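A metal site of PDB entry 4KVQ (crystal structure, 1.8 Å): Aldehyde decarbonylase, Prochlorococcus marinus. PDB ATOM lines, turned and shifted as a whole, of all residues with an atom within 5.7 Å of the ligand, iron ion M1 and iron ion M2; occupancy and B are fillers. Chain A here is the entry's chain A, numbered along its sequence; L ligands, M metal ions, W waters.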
ATOM      1  N   TYR A  35       4.404  14.173  19.873  1.00  0.00           N
ATOM      2  CA  TYR A  35       5.668  13.534  19.477  1.00  0.00           C
ATOM      3  C   TYR A  35       6.851  14.386  19.921  1.00  0.00           C
ATOM      4  O   TYR A  35       7.904  13.845  20.244  1.00  0.00           O
ATOM      5  CB  TYR A  35       5.709  13.284  17.967  1.00  0.00           C
ATOM      6  CG  TYR A  35       6.632  12.122  17.573  1.00  0.00           C
ATOM      7  CD1 TYR A  35       6.189  10.811  17.629  1.00  0.00           C
ATOM      8  CD2 TYR A  35       7.944  12.353  17.158  1.00  0.00           C
ATOM      9  CE1 TYR A  35       7.026   9.746  17.290  1.00  0.00           C
ATOM     10  CE2 TYR A  35       8.782  11.300  16.800  1.00  0.00           C
ATOM     11  CZ  TYR A  35       8.315  10.000  16.873  1.00  0.00           C
ATOM     12  OH  TYR A  35       9.131   8.948  16.519  1.00  0.00           O
ATOM     13  N   ILE A  38       7.435  13.162  23.498  1.00  0.00           N
ATOM     14  CA  ILE A  38       7.793  11.738  23.567  1.00  0.00           C
ATOM     15  C   ILE A  38       9.167  11.480  22.929  1.00  0.00           C
ATOM     16  O   ILE A  38      10.007  10.771  23.490  1.00  0.00           O
ATOM     17  CB  ILE A  38       6.758  10.877  22.845  1.00  0.00           C
ATOM     18  CG1 ILE A  38       5.417  10.953  23.558  1.00  0.00           C
ATOM     19  CG2 ILE A  38       7.217   9.401  22.752  1.00  0.00           C
ATOM     20  CD1 ILE A  38       5.493  10.509  24.952  1.00  0.00           C
ATOM     21  N   ILE A  41      11.881  12.742  25.234  1.00  0.00           N
ATOM     22  CA  ILE A  41      12.092  11.840  26.365  1.00  0.00           C
ATOM     23  C   ILE A  41      12.951  10.644  25.967  1.00  0.00           C
ATOM     24  O   ILE A  41      13.870  10.276  26.698  1.00  0.00           O
ATOM     25  CB  ILE A  41      10.728  11.362  26.952  1.00  0.00           C
ATOM     26  CG1 ILE A  41      10.091  12.500  27.753  1.00  0.00           C
ATOM     27  CG2 ILE A  41      10.911  10.144  27.846  1.00  0.00           C
ATOM     28  CD1 ILE A  41       8.656  12.218  28.192  1.00  0.00           C
ATOM     29  N   VAL A  42      12.674  10.067  24.810  1.00  0.00           N
ATOM     30  CA  VAL A  42      13.474   8.930  24.341  1.00  0.00           C
ATOM     31  C   VAL A  42      14.934   9.356  24.067  1.00  0.00           C
ATOM     32  O   VAL A  42      15.871   8.677  24.470  1.00  0.00           O
ATOM     33  CB  VAL A  42      12.823   8.272  23.107  1.00  0.00           C
ATOM     34  CG1 VAL A  42      13.721   7.214  22.561  1.00  0.00           C
ATOM     35  CG2 VAL A  42      11.461   7.662  23.484  1.00  0.00           C
ATOM     36  N   GLY A  45      16.601   9.899  27.331  1.00  0.00           N
ATOM     37  CA  GLY A  45      16.776   8.645  28.014  1.00  0.00           C
ATOM     38  C   GLY A  45      17.964   7.866  27.472  1.00  0.00           C
ATOM     39  O   GLY A  45      18.698   7.241  28.244  1.00  0.00           O
ATOM     40  N   GLU A  46      18.126   7.864  26.160  1.00  0.00           N
ATOM     41  CA  GLU A  46      19.261   7.187  25.533  1.00  0.00           C
ATOM     42  C   GLU A  46      20.572   7.840  25.928  1.00  0.00           C
ATOM     43  O   GLU A  46      21.549   7.163  26.179  1.00  0.00           O
ATOM     44  CB  GLU A  46      19.110   7.161  24.007  1.00  0.00           C
ATOM     45  CG  GLU A  46      17.854   6.442  23.518  1.00  0.00           C
ATOM     46  CD  GLU A  46      17.912   4.936  23.733  1.00  0.00           C
ATOM     47  OE1 GLU A  46      18.997   4.431  24.108  1.00  0.00           O
ATOM     48  OE2 GLU A  46      16.882   4.257  23.528  1.00  0.00           O
ATOM     49  N   ALA A  49      21.229   6.821  29.435  1.00  0.00           N
ATOM     50  CA  ALA A  49      21.671   5.424  29.473  1.00  0.00           C
ATOM     51  C   ALA A  49      23.162   5.362  29.147  1.00  0.00           C
ATOM     52  O   ALA A  49      23.931   4.691  29.842  1.00  0.00           O
ATOM     53  CB  ALA A  49      20.845   4.564  28.504  1.00  0.00           C
ATOM     54  N   TYR A  53      25.974   3.958  31.906  1.00  0.00           N
ATOM     55  CA  TYR A  53      26.865   2.819  31.729  1.00  0.00           C
ATOM     56  C   TYR A  53      28.336   3.252  31.848  1.00  0.00           C
ATOM     57  O   TYR A  53      29.135   2.540  32.436  1.00  0.00           O
ATOM     58  CB  TYR A  53      26.596   2.069  30.416  1.00  0.00           C
ATOM     59  CG  TYR A  53      25.317   1.272  30.475  1.00  0.00           C
ATOM     60  CD1 TYR A  53      25.128   0.298  31.453  1.00  0.00           C
ATOM     61  CD2 TYR A  53      24.283   1.488  29.563  1.00  0.00           C
ATOM     62  CE1 TYR A  53      23.950  -0.439  31.524  1.00  0.00           C
ATOM     63  CE2 TYR A  53      23.101   0.742  29.634  1.00  0.00           C
ATOM     64  CZ  TYR A  53      22.949  -0.207  30.619  1.00  0.00           C
ATOM     65  OH  TYR A  53      21.777  -0.936  30.691  1.00  0.00           O
ATOM     66  N   MET A  73      26.195   1.656  22.088  1.00  0.00           N
ATOM     67  CA  MET A  73      24.895   1.268  21.553  1.00  0.00           C
ATOM     68  C   MET A  73      23.858   2.337  21.869  1.00  0.00           C
ATOM     69  O   MET A  73      23.011   2.653  21.032  1.00  0.00           O
ATOM     70  CB  MET A  73      24.410  -0.084  22.106  1.00  0.00           C
ATOM     71  CG  MET A  73      25.288  -1.285  21.786  1.00  0.00           C
ATOM     72  SD  MET A  73      24.578  -2.802  22.486  1.00  0.00           S
ATOM     73  CE  MET A  73      25.999  -3.906  22.370  1.00  0.00           C
ATOM     74  N   GLU A  74      23.911   2.867  23.091  1.00  0.00           N
ATOM     75  CA  GLU A  74      22.944   3.881  23.508  1.00  0.00           C
ATOM     76  C   GLU A  74      23.073   5.116  22.629  1.00  0.00           C
ATOM     77  O   GLU A  74      22.075   5.753  22.292  1.00  0.00           O
ATOM     78  CB  GLU A  74      23.102   4.245  24.990  1.00  0.00           C
ATOM     79  CG  GLU A  74      23.004   3.043  25.961  1.00  0.00           C
ATOM     80  CD  GLU A  74      21.641   2.339  25.970  1.00  0.00           C
ATOM     81  OE1 GLU A  74      20.860   2.483  25.018  1.00  0.00           O
ATOM     82  OE2 GLU A  74      21.363   1.603  26.945  1.00  0.00           O
ATOM     83  N   HIS A  77      21.280   4.440  19.439  1.00  0.00           N
ATOM     84  CA  HIS A  77      19.825   4.572  19.646  1.00  0.00           C
ATOM     85  C   HIS A  77      19.434   6.053  19.644  1.00  0.00           C
ATOM     86  O   HIS A  77      18.447   6.447  19.034  1.00  0.00           O
ATOM     87  CB  HIS A  77      19.410   3.957  20.989  1.00  0.00           C
ATOM     88  CG  HIS A  77      19.784   2.517  21.146  1.00  0.00           C
ATOM     89  ND1 HIS A  77      19.675   1.856  22.350  1.00  0.00           N
ATOM     90  CD2 HIS A  77      20.242   1.603  20.254  1.00  0.00           C
ATOM     91  CE1 HIS A  77      20.068   0.600  22.206  1.00  0.00           C
ATOM     92  NE2 HIS A  77      20.422   0.426  20.940  1.00  0.00           N
ATOM     93  N   PHE A  81      16.732   7.798  17.122  1.00  0.00           N
ATOM     94  CA  PHE A  81      15.493   8.443  17.555  1.00  0.00           C
ATOM     95  C   PHE A  81      15.505   9.931  17.251  1.00  0.00           C
ATOM     96  O   PHE A  81      14.470  10.527  16.976  1.00  0.00           O
ATOM     97  CB  PHE A  81      15.243   8.150  19.039  1.00  0.00           C
ATOM     98  CG  PHE A  81      14.851   6.727  19.313  1.00  0.00           C
ATOM     99  CD1 PHE A  81      13.803   6.154  18.603  1.00  0.00           C
ATOM    100  CD2 PHE A  81      15.519   5.954  20.236  1.00  0.00           C
ATOM    101  CE1 PHE A  81      13.425   4.829  18.831  1.00  0.00           C
ATOM    102  CE2 PHE A  81      15.136   4.631  20.486  1.00  0.00           C
ATOM    103  CZ  PHE A  81      14.097   4.076  19.778  1.00  0.00           C
ATOM    104  N   PHE A 100      11.633  15.441  33.092  1.00  0.00           N
ATOM    105  CA  PHE A 100      11.014  14.116  33.200  1.00  0.00           C
ATOM    106  C   PHE A 100      11.944  13.114  33.866  1.00  0.00           C
ATOM    107  O   PHE A 100      11.502  12.317  34.697  1.00  0.00           O
ATOM    108  CB  PHE A 100      10.647  13.640  31.789  1.00  0.00           C
ATOM    109  CG  PHE A 100       9.973  12.300  31.729  1.00  0.00           C
ATOM    110  CD1 PHE A 100       8.607  12.166  31.985  1.00  0.00           C
ATOM    111  CD2 PHE A 100      10.683  11.170  31.340  1.00  0.00           C
ATOM    112  CE1 PHE A 100       7.989  10.937  31.882  1.00  0.00           C
ATOM    113  CE2 PHE A 100      10.064   9.941  31.237  1.00  0.00           C
ATOM    114  CZ  PHE A 100       8.708   9.825  31.495  1.00  0.00           C
ATOM    115  N   PHE A 101      13.219  13.136  33.483  1.00  0.00           N
ATOM    116  CA  PHE A 101      14.226  12.208  34.004  1.00  0.00           C
ATOM    117  C   PHE A 101      14.915  12.662  35.288  1.00  0.00           C
ATOM    118  O   PHE A 101      15.613  11.864  35.912  1.00  0.00           O
ATOM    119  CB  PHE A 101      15.291  11.907  32.952  1.00  0.00           C
ATOM    120  CG  PHE A 101      14.873  10.845  31.994  1.00  0.00           C
ATOM    121  CD1 PHE A 101      14.899   9.523  32.383  1.00  0.00           C
ATOM    122  CD2 PHE A 101      14.435  11.164  30.718  1.00  0.00           C
ATOM    123  CE1 PHE A 101      14.492   8.528  31.507  1.00  0.00           C
ATOM    124  CE2 PHE A 101      14.021  10.171  29.855  1.00  0.00           C
ATOM    125  CZ  PHE A 101      14.051   8.858  30.244  1.00  0.00           C
ATOM    126  N   GLN A 124      19.439   1.599  36.147  1.00  0.00           N
ATOM    127  CA  GLN A 124      19.627   1.672  34.709  1.00  0.00           C
ATOM    128  C   GLN A 124      19.319   0.363  34.006  1.00  0.00           C
ATOM    129  O   GLN A 124      18.496   0.334  33.092  1.00  0.00           O
ATOM    130  CB  GLN A 124      21.049   2.103  34.329  1.00  0.00           C
ATOM    131  CG  GLN A 124      21.303   1.969  32.800  1.00  0.00           C
ATOM    132  CD  GLN A 124      20.400   2.846  31.960  1.00  0.00           C
ATOM    133  OE1 GLN A 124      20.185   4.018  32.273  1.00  0.00           O
ATOM    134  NE2 GLN A 124      19.857   2.278  30.866  1.00  0.00           N
ATOM    135  N   ILE A 128      15.113   1.131  33.992  1.00  0.00           N
ATOM    136  CA  ILE A 128      15.074   1.939  32.779  1.00  0.00           C
ATOM    137  C   ILE A 128      15.062   1.073  31.521  1.00  0.00           C
ATOM    138  O   ILE A 128      14.299   1.352  30.600  1.00  0.00           O
ATOM    139  CB  ILE A 128      16.185   3.000  32.758  1.00  0.00           C
ATOM    140  CG1 ILE A 128      15.953   4.003  33.891  1.00  0.00           C
ATOM    141  CG2 ILE A 128      16.197   3.722  31.428  1.00  0.00           C
ATOM    142  CD1 ILE A 128      17.023   5.063  34.012  1.00  0.00           C
ATOM    143  N   GLU A 129      15.851  -0.001  31.478  1.00  0.00           N
ATOM    144  CA  GLU A 129      15.814  -0.872  30.306  1.00  0.00           C
ATOM    145  C   GLU A 129      14.439  -1.533  30.149  1.00  0.00           C
ATOM    146  O   GLU A 129      13.922  -1.605  29.046  1.00  0.00           O
ATOM    147  CB  GLU A 129      16.893  -1.956  30.331  1.00  0.00           C
ATOM    148  CG  GLU A 129      18.329  -1.453  30.365  1.00  0.00           C
ATOM    149  CD  GLU A 129      18.790  -0.776  29.075  1.00  0.00           C
ATOM    150  OE1 GLU A 129      18.119  -0.907  28.022  1.00  0.00           O
ATOM    151  OE2 GLU A 129      19.872  -0.121  29.101  1.00  0.00           O
ATOM    152  N   PHE A 131      11.574  -0.314  31.160  1.00  0.00           N
ATOM    153  CA  PHE A 131      10.662   0.759  30.761  1.00  0.00           C
ATOM    154  C   PHE A 131      10.806   0.997  29.247  1.00  0.00           C
ATOM    155  O   PHE A 131       9.822   1.093  28.521  1.00  0.00           O
ATOM    156  CB  PHE A 131      11.009   2.017  31.572  1.00  0.00           C
ATOM    157  CG  PHE A 131      10.057   3.173  31.380  1.00  0.00           C
ATOM    158  CD1 PHE A 131       8.806   2.988  30.820  1.00  0.00           C
ATOM    159  CD2 PHE A 131      10.433   4.450  31.765  1.00  0.00           C
ATOM    160  CE1 PHE A 131       7.937   4.065  30.651  1.00  0.00           C
ATOM    161  CE2 PHE A 131       9.577   5.531  31.594  1.00  0.00           C
ATOM    162  CZ  PHE A 131       8.330   5.333  31.031  1.00  0.00           C
ATOM    163  N   ALA A 132      12.052   1.052  28.782  1.00  0.00           N
ATOM    164  CA  ALA A 132      12.323   1.239  27.358  1.00  0.00           C
ATOM    165  C   ALA A 132      11.773   0.101  26.515  1.00  0.00           C
ATOM    166  O   ALA A 132      11.129   0.326  25.499  1.00  0.00           O
ATOM    167  CB  ALA A 132      13.820   1.372  27.118  1.00  0.00           C
ATOM    168  N   ALA A 135       8.040   0.285  26.348  1.00  0.00           N
ATOM    169  CA  ALA A 135       7.636   1.432  25.534  1.00  0.00           C
ATOM    170  C   ALA A 135       7.887   1.170  24.055  1.00  0.00           C
ATOM    171  O   ALA A 135       7.013   1.410  23.220  1.00  0.00           O
ATOM    172  CB  ALA A 135       8.375   2.661  25.986  1.00  0.00           C
ATOM    173  N   TYR A 136       9.073   0.680  23.732  1.00  0.00           N
ATOM    174  CA  TYR A 136       9.383   0.427  22.325  1.00  0.00           C
ATOM    175  C   TYR A 136       8.500  -0.658  21.720  1.00  0.00           C
ATOM    176  O   TYR A 136       8.036  -0.518  20.593  1.00  0.00           O
ATOM    177  CB  TYR A 136      10.879   0.102  22.158  1.00  0.00           C
ATOM    178  CG  TYR A 136      11.801   1.226  22.587  1.00  0.00           C
ATOM    179  CD1 TYR A 136      11.338   2.531  22.723  1.00  0.00           C
ATOM    180  CD2 TYR A 136      13.137   0.970  22.877  1.00  0.00           C
ATOM    181  CE1 TYR A 136      12.184   3.561  23.129  1.00  0.00           C
ATOM    182  CE2 TYR A 136      13.998   2.003  23.291  1.00  0.00           C
ATOM    183  CZ  TYR A 136      13.504   3.280  23.406  1.00  0.00           C
ATOM    184  OH  TYR A 136      14.343   4.291  23.821  1.00  0.00           O
ATOM    185  N   TYR A 139       5.126   0.884  21.035  1.00  0.00           N
ATOM    186  CA  TYR A 139       5.162   1.877  19.966  1.00  0.00           C
ATOM    187  C   TYR A 139       5.260   1.259  18.576  1.00  0.00           C
ATOM    188  O   TYR A 139       4.682   1.783  17.632  1.00  0.00           O
ATOM    189  CB  TYR A 139       6.341   2.816  20.199  1.00  0.00           C
ATOM    190  CG  TYR A 139       6.648   3.817  19.101  1.00  0.00           C
ATOM    191  CD1 TYR A 139       5.721   4.784  18.716  1.00  0.00           C
ATOM    192  CD2 TYR A 139       7.919   3.859  18.505  1.00  0.00           C
ATOM    193  CE1 TYR A 139       6.021   5.723  17.742  1.00  0.00           C
ATOM    194  CE2 TYR A 139       8.224   4.806  17.531  1.00  0.00           C
ATOM    195  CZ  TYR A 139       7.275   5.727  17.153  1.00  0.00           C
ATOM    196  OH  TYR A 139       7.586   6.660  16.186  1.00  0.00           O
ATOM    197  N   THR A 151      13.137   1.600  15.569  1.00  0.00           N
ATOM    198  CA  THR A 151      12.761   1.049  16.854  1.00  0.00           C
ATOM    199  C   THR A 151      12.932  -0.470  16.922  1.00  0.00           C
ATOM    200  O   THR A 151      13.352  -1.008  17.944  1.00  0.00           O
ATOM    201  CB  THR A 151      11.308   1.437  17.231  1.00  0.00           C
ATOM    202  OG1 THR A 151      11.118   2.852  17.034  1.00  0.00           O
ATOM    203  CG2 THR A 151      11.022   1.085  18.690  1.00  0.00           C
ATOM    204  N   VAL A 154      16.504  -1.136  17.663  1.00  0.00           N
ATOM    205  CA  VAL A 154      16.897  -0.795  19.035  1.00  0.00           C
ATOM    206  C   VAL A 154      16.485  -1.849  20.061  1.00  0.00           C
ATOM    207  O   VAL A 154      17.240  -2.148  20.990  1.00  0.00           O
ATOM    208  CB  VAL A 154      16.301   0.580  19.435  1.00  0.00           C
ATOM    209  CG1 VAL A 154      16.330   0.760  20.950  1.00  0.00           C
ATOM    210  CG2 VAL A 154      17.057   1.723  18.742  1.00  0.00           C
ATOM    211  N   ASP A 157      18.857  -4.599  21.175  1.00  0.00           N
ATOM    212  CA  ASP A 157      19.952  -4.153  22.028  1.00  0.00           C
ATOM    213  C   ASP A 157      19.528  -4.059  23.479  1.00  0.00           C
ATOM    214  O   ASP A 157      20.334  -4.314  24.386  1.00  0.00           O
ATOM    215  CB  ASP A 157      20.484  -2.779  21.604  1.00  0.00           C
ATOM    216  CG  ASP A 157      21.352  -2.839  20.364  1.00  0.00           C
ATOM    217  OD1 ASP A 157      21.726  -3.962  19.958  1.00  0.00           O
ATOM    218  OD2 ASP A 157      21.669  -1.762  19.825  1.00  0.00           O
ATOM    219  N   GLU A 158      18.285  -3.669  23.734  1.00  0.00           N
ATOM    220  CA  GLU A 158      17.909  -3.427  25.130  1.00  0.00           C
ATOM    221  C   GLU A 158      17.815  -4.762  25.901  1.00  0.00           C
ATOM    222  O   GLU A 158      18.044  -4.797  27.112  1.00  0.00           O
ATOM    223  CB  GLU A 158      16.654  -2.535  25.270  1.00  0.00           C
ATOM    224  CG  GLU A 158      16.593  -1.285  24.307  1.00  0.00           C
ATOM    225  CD  GLU A 158      17.581  -0.103  24.579  1.00  0.00           C
ATOM    226  OE1 GLU A 158      17.242   1.046  24.156  1.00  0.00           O
ATOM    227  OE2 GLU A 158      18.685  -0.273  25.165  1.00  0.00           O
ATOM    228  N   HIS A 161      21.102  -5.374  27.255  1.00  0.00           N
ATOM    229  CA  HIS A 161      21.430  -4.515  28.380  1.00  0.00           C
ATOM    230  C   HIS A 161      20.822  -5.080  29.645  1.00  0.00           C
ATOM    231  O   HIS A 161      21.475  -5.142  30.688  1.00  0.00           O
ATOM    232  CB  HIS A 161      20.933  -3.092  28.098  1.00  0.00           C
ATOM    233  CG  HIS A 161      21.592  -2.448  26.920  1.00  0.00           C
ATOM    234  ND1 HIS A 161      21.198  -1.231  26.428  1.00  0.00           N
ATOM    235  CD2 HIS A 161      22.611  -2.861  26.147  1.00  0.00           C
ATOM    236  CE1 HIS A 161      21.951  -0.919  25.390  1.00  0.00           C
ATOM    237  NE2 HIS A 161      22.823  -1.900  25.193  1.00  0.00           N
ATOM    238  N   VAL A 198       3.652  10.310  31.086  1.00  0.00           N
ATOM    239  CA  VAL A 198       3.793  10.126  29.651  1.00  0.00           C
ATOM    240  C   VAL A 198       2.482   9.663  29.001  1.00  0.00           C
ATOM    241  O   VAL A 198       2.313   9.735  27.775  1.00  0.00           O
ATOM    242  CB  VAL A 198       4.951   9.137  29.378  1.00  0.00           C
ATOM    243  CG1 VAL A 198       4.444   7.708  29.208  1.00  0.00           C
ATOM    244  CG2 VAL A 198       5.771   9.573  28.194  1.00  0.00           C
ATOM    245  N   ALA A 202       1.391   9.616  25.097  1.00  0.00           N
ATOM    246  CA  ALA A 202       1.426   8.263  24.548  1.00  0.00           C
ATOM    247  C   ALA A 202       0.102   7.885  23.905  1.00  0.00           C
ATOM    248  O   ALA A 202       0.087   7.207  22.877  1.00  0.00           O
ATOM    249  CB  ALA A 202       1.834   7.229  25.629  1.00  0.00           C
ATOM    250  N   LEU A 205      -0.258   9.100  20.532  1.00  0.00           N
ATOM    251  CA  LEU A 205       0.529   8.228  19.669  1.00  0.00           C
ATOM    252  C   LEU A 205      -0.111   6.847  19.471  1.00  0.00           C
ATOM    253  O   LEU A 205       0.498   5.955  18.875  1.00  0.00           O
ATOM    254  CB  LEU A 205       1.956   8.085  20.209  1.00  0.00           C
ATOM    255  CG  LEU A 205       3.012   9.088  19.723  1.00  0.00           C
ATOM    256  CD1 LEU A 205       2.636  10.528  20.011  1.00  0.00           C
ATOM    257  CD2 LEU A 205       4.350   8.768  20.383  1.00  0.00           C
ATOM    258  N   MET A 207      -0.879   4.663  21.820  1.00  0.00           N
ATOM    259  CA  MET A 207      -0.362   3.674  22.754  1.00  0.00           C
ATOM    260  C   MET A 207      -1.244   3.627  24.009  1.00  0.00           C
ATOM    261  O   MET A 207      -1.546   4.665  24.582  1.00  0.00           O
ATOM    262  CB  MET A 207       1.068   4.040  23.137  1.00  0.00           C
ATOM    263  CG  MET A 207       2.028   4.032  21.929  1.00  0.00           C
ATOM    264  SD  MET A 207       3.631   4.782  22.327  1.00  0.00           S
ATOM    265  CE  MET A 207       4.224   3.579  23.467  1.00  0.00           C
ATOM    266  N   LEU A 212       1.552  -0.392  28.328  1.00  0.00           N
ATOM    267  CA  LEU A 212       2.836   0.110  28.815  1.00  0.00           C
ATOM    268  C   LEU A 212       3.136  -0.419  30.213  1.00  0.00           C
ATOM    269  O   LEU A 212       4.232  -0.899  30.498  1.00  0.00           O
ATOM    270  CB  LEU A 212       2.860   1.635  28.815  1.00  0.00           C
ATOM    271  CG  LEU A 212       2.974   2.360  27.476  1.00  0.00           C
ATOM    272  CD1 LEU A 212       2.835   3.877  27.650  1.00  0.00           C
ATOM    273  CD2 LEU A 212       4.310   2.033  26.822  1.00  0.00           C
HETATM  274  C1  LIG L   1      18.023   2.616  27.286  1.00  0.00           C
HETATM  275  O1  LIG L   1      18.679   2.096  26.397  1.00  0.00           O
HETATM  276  O2  LIG L   1      18.049   2.368  28.518  1.00  0.00           O
HETATM  277  C2  LIG L   1      17.027   3.705  26.802  1.00  0.00           C
HETATM  278  C3  LIG L   1      16.156   4.310  27.882  1.00  0.00           C
HETATM  279  C4  LIG L   1      15.118   5.332  27.374  1.00  0.00           C
HETATM  280  C5  LIG L   1      13.793   5.317  28.140  1.00  0.00           C
HETATM  281  C6  LIG L   1      12.574   5.672  27.267  1.00  0.00           C
HETATM  282  C7  LIG L   1      11.221   5.630  27.982  1.00  0.00           C
HETATM  283  C8  LIG L   1      10.158   6.541  27.334  1.00  0.00           C
HETATM  284  C9  LIG L   1       8.750   5.955  27.301  1.00  0.00           C
HETATM  285  C10 LIG L   1       7.713   6.857  26.595  1.00  0.00           C
HETATM  286  C11 LIG L   1       7.074   6.241  25.324  1.00  0.00           C
HETATM  287  C12 LIG L   1       8.046   6.225  24.134  1.00  0.00           C
HETATM  288  C13 LIG L   1       7.528   5.473  22.920  1.00  0.00           C
HETATM  289  C14 LIG L   1       8.641   5.155  21.907  1.00  0.00           C
HETATM  290  C15 LIG L   1       8.919   6.287  20.920  1.00  0.00           C
HETATM  291  C16 LIG L   1      10.195   6.036  20.126  1.00  0.00           C
HETATM  292 FE    FE M   1      18.952   2.364  24.377  1.00  0.00          FE
HETATM  293 FE    FE M   2      19.711   0.360  26.964  1.00  0.00          FE
HETATM  294  O   HOH W   1      11.077   8.695  19.153  1.00  0.00           O
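The side-chain amide nitrogen of Gln 124 lies within hydrogen-bond range of an oxygen (O2) of the ligand (3.0 Å).
The side-chain carboxylate of Glu 46 is in hydrogen-bond range of the side-chain hydroxyl of Tyr 136 (2.6 Å).
OE2 of Glu 129 lies close to OH of Tyr 53.
A ring nitrogen (NE2) of His 77 sits close to the backbone carbonyl oxygen (O) of Met 73, 3.4 Å away.
OH of Tyr 139 is in hydrogen-bond range of OH of Tyr 35 (2.8 Å).
N of Glu 129 lies within hydrogen-bond range of O of Gln 124 (3.1 Å).
A ring nitrogen (NE2) of His 77 lies within hydrogen-bond range of the side-chain carboxylate (OD2) of Asp 157, at 2.8 Å.
N of Met 207 sits at hydrogen-bond distance from O of Ala 202, 2.9 Å away.
NE2 of His 161 lies within hydrogen-bond range of SD of Met 73, 3.3 Å away.
Merely in contact with the ligand: Ile 38 (3.6 Å), Ile 41 (3.7 Å), Val 42 (3.8 Å), Gly 45 (3.8 Å), Ala 49 (3.6 Å), Phe 81 (3.7 Å), Ile 128 (3.6 Å), Phe 131 (3.8 Å), Ala 132 (3.8 Å), Ala 135 (3.6 Å), Tyr 136 (3.8 Å), Tyr 139 (3.5 Å), Val 198 (3.7 Å) and Met 207 (3.8 Å).
Within 4 Å of the ligand: Ile 38, Ile 41, Val 42, Gly 45, Glu 46, Ala 49, Glu 74, Phe 81, Gln 124, Ile 128, Glu 129, Phe 131, Ala 132, Ala 135, Tyr 136, Tyr 139, Glu 158, Val 198 and Met 207.
Along chain A the residues within 4 Å of the ligand span positions 38 to 207.
The nearest printed residue that does not touch the ligand is Phe 101 (4.1 Å).
Within 4 Å of iron ion M1: Glu 46, Glu 74, His 77 and Glu 158.
Of the 32 residues printed, 4 come within 4 Å of iron ion M2.
Iron ion M1 is bound by OE1 of Glu 74 (2.0 Å), O1 of the ligand (2.1 Å), OE1 of Glu 46 (2.1 Å), OE1 of Glu 158 (2.2 Å) and ND1 of His 77 (2.2 Å).
Iron ion M1 has five donor atoms within binding distance.
Slightly farther from iron ion M1 lies the side-chain carboxylate (OE2) of Glu 158 (2.8 Å).
Iron ion M2 is bound by OE2 of Glu 74, O1 of the ligand, OE2 of Glu 158, OE2 of Glu 129, ND1 of His 161 and OE1 of Glu 129.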
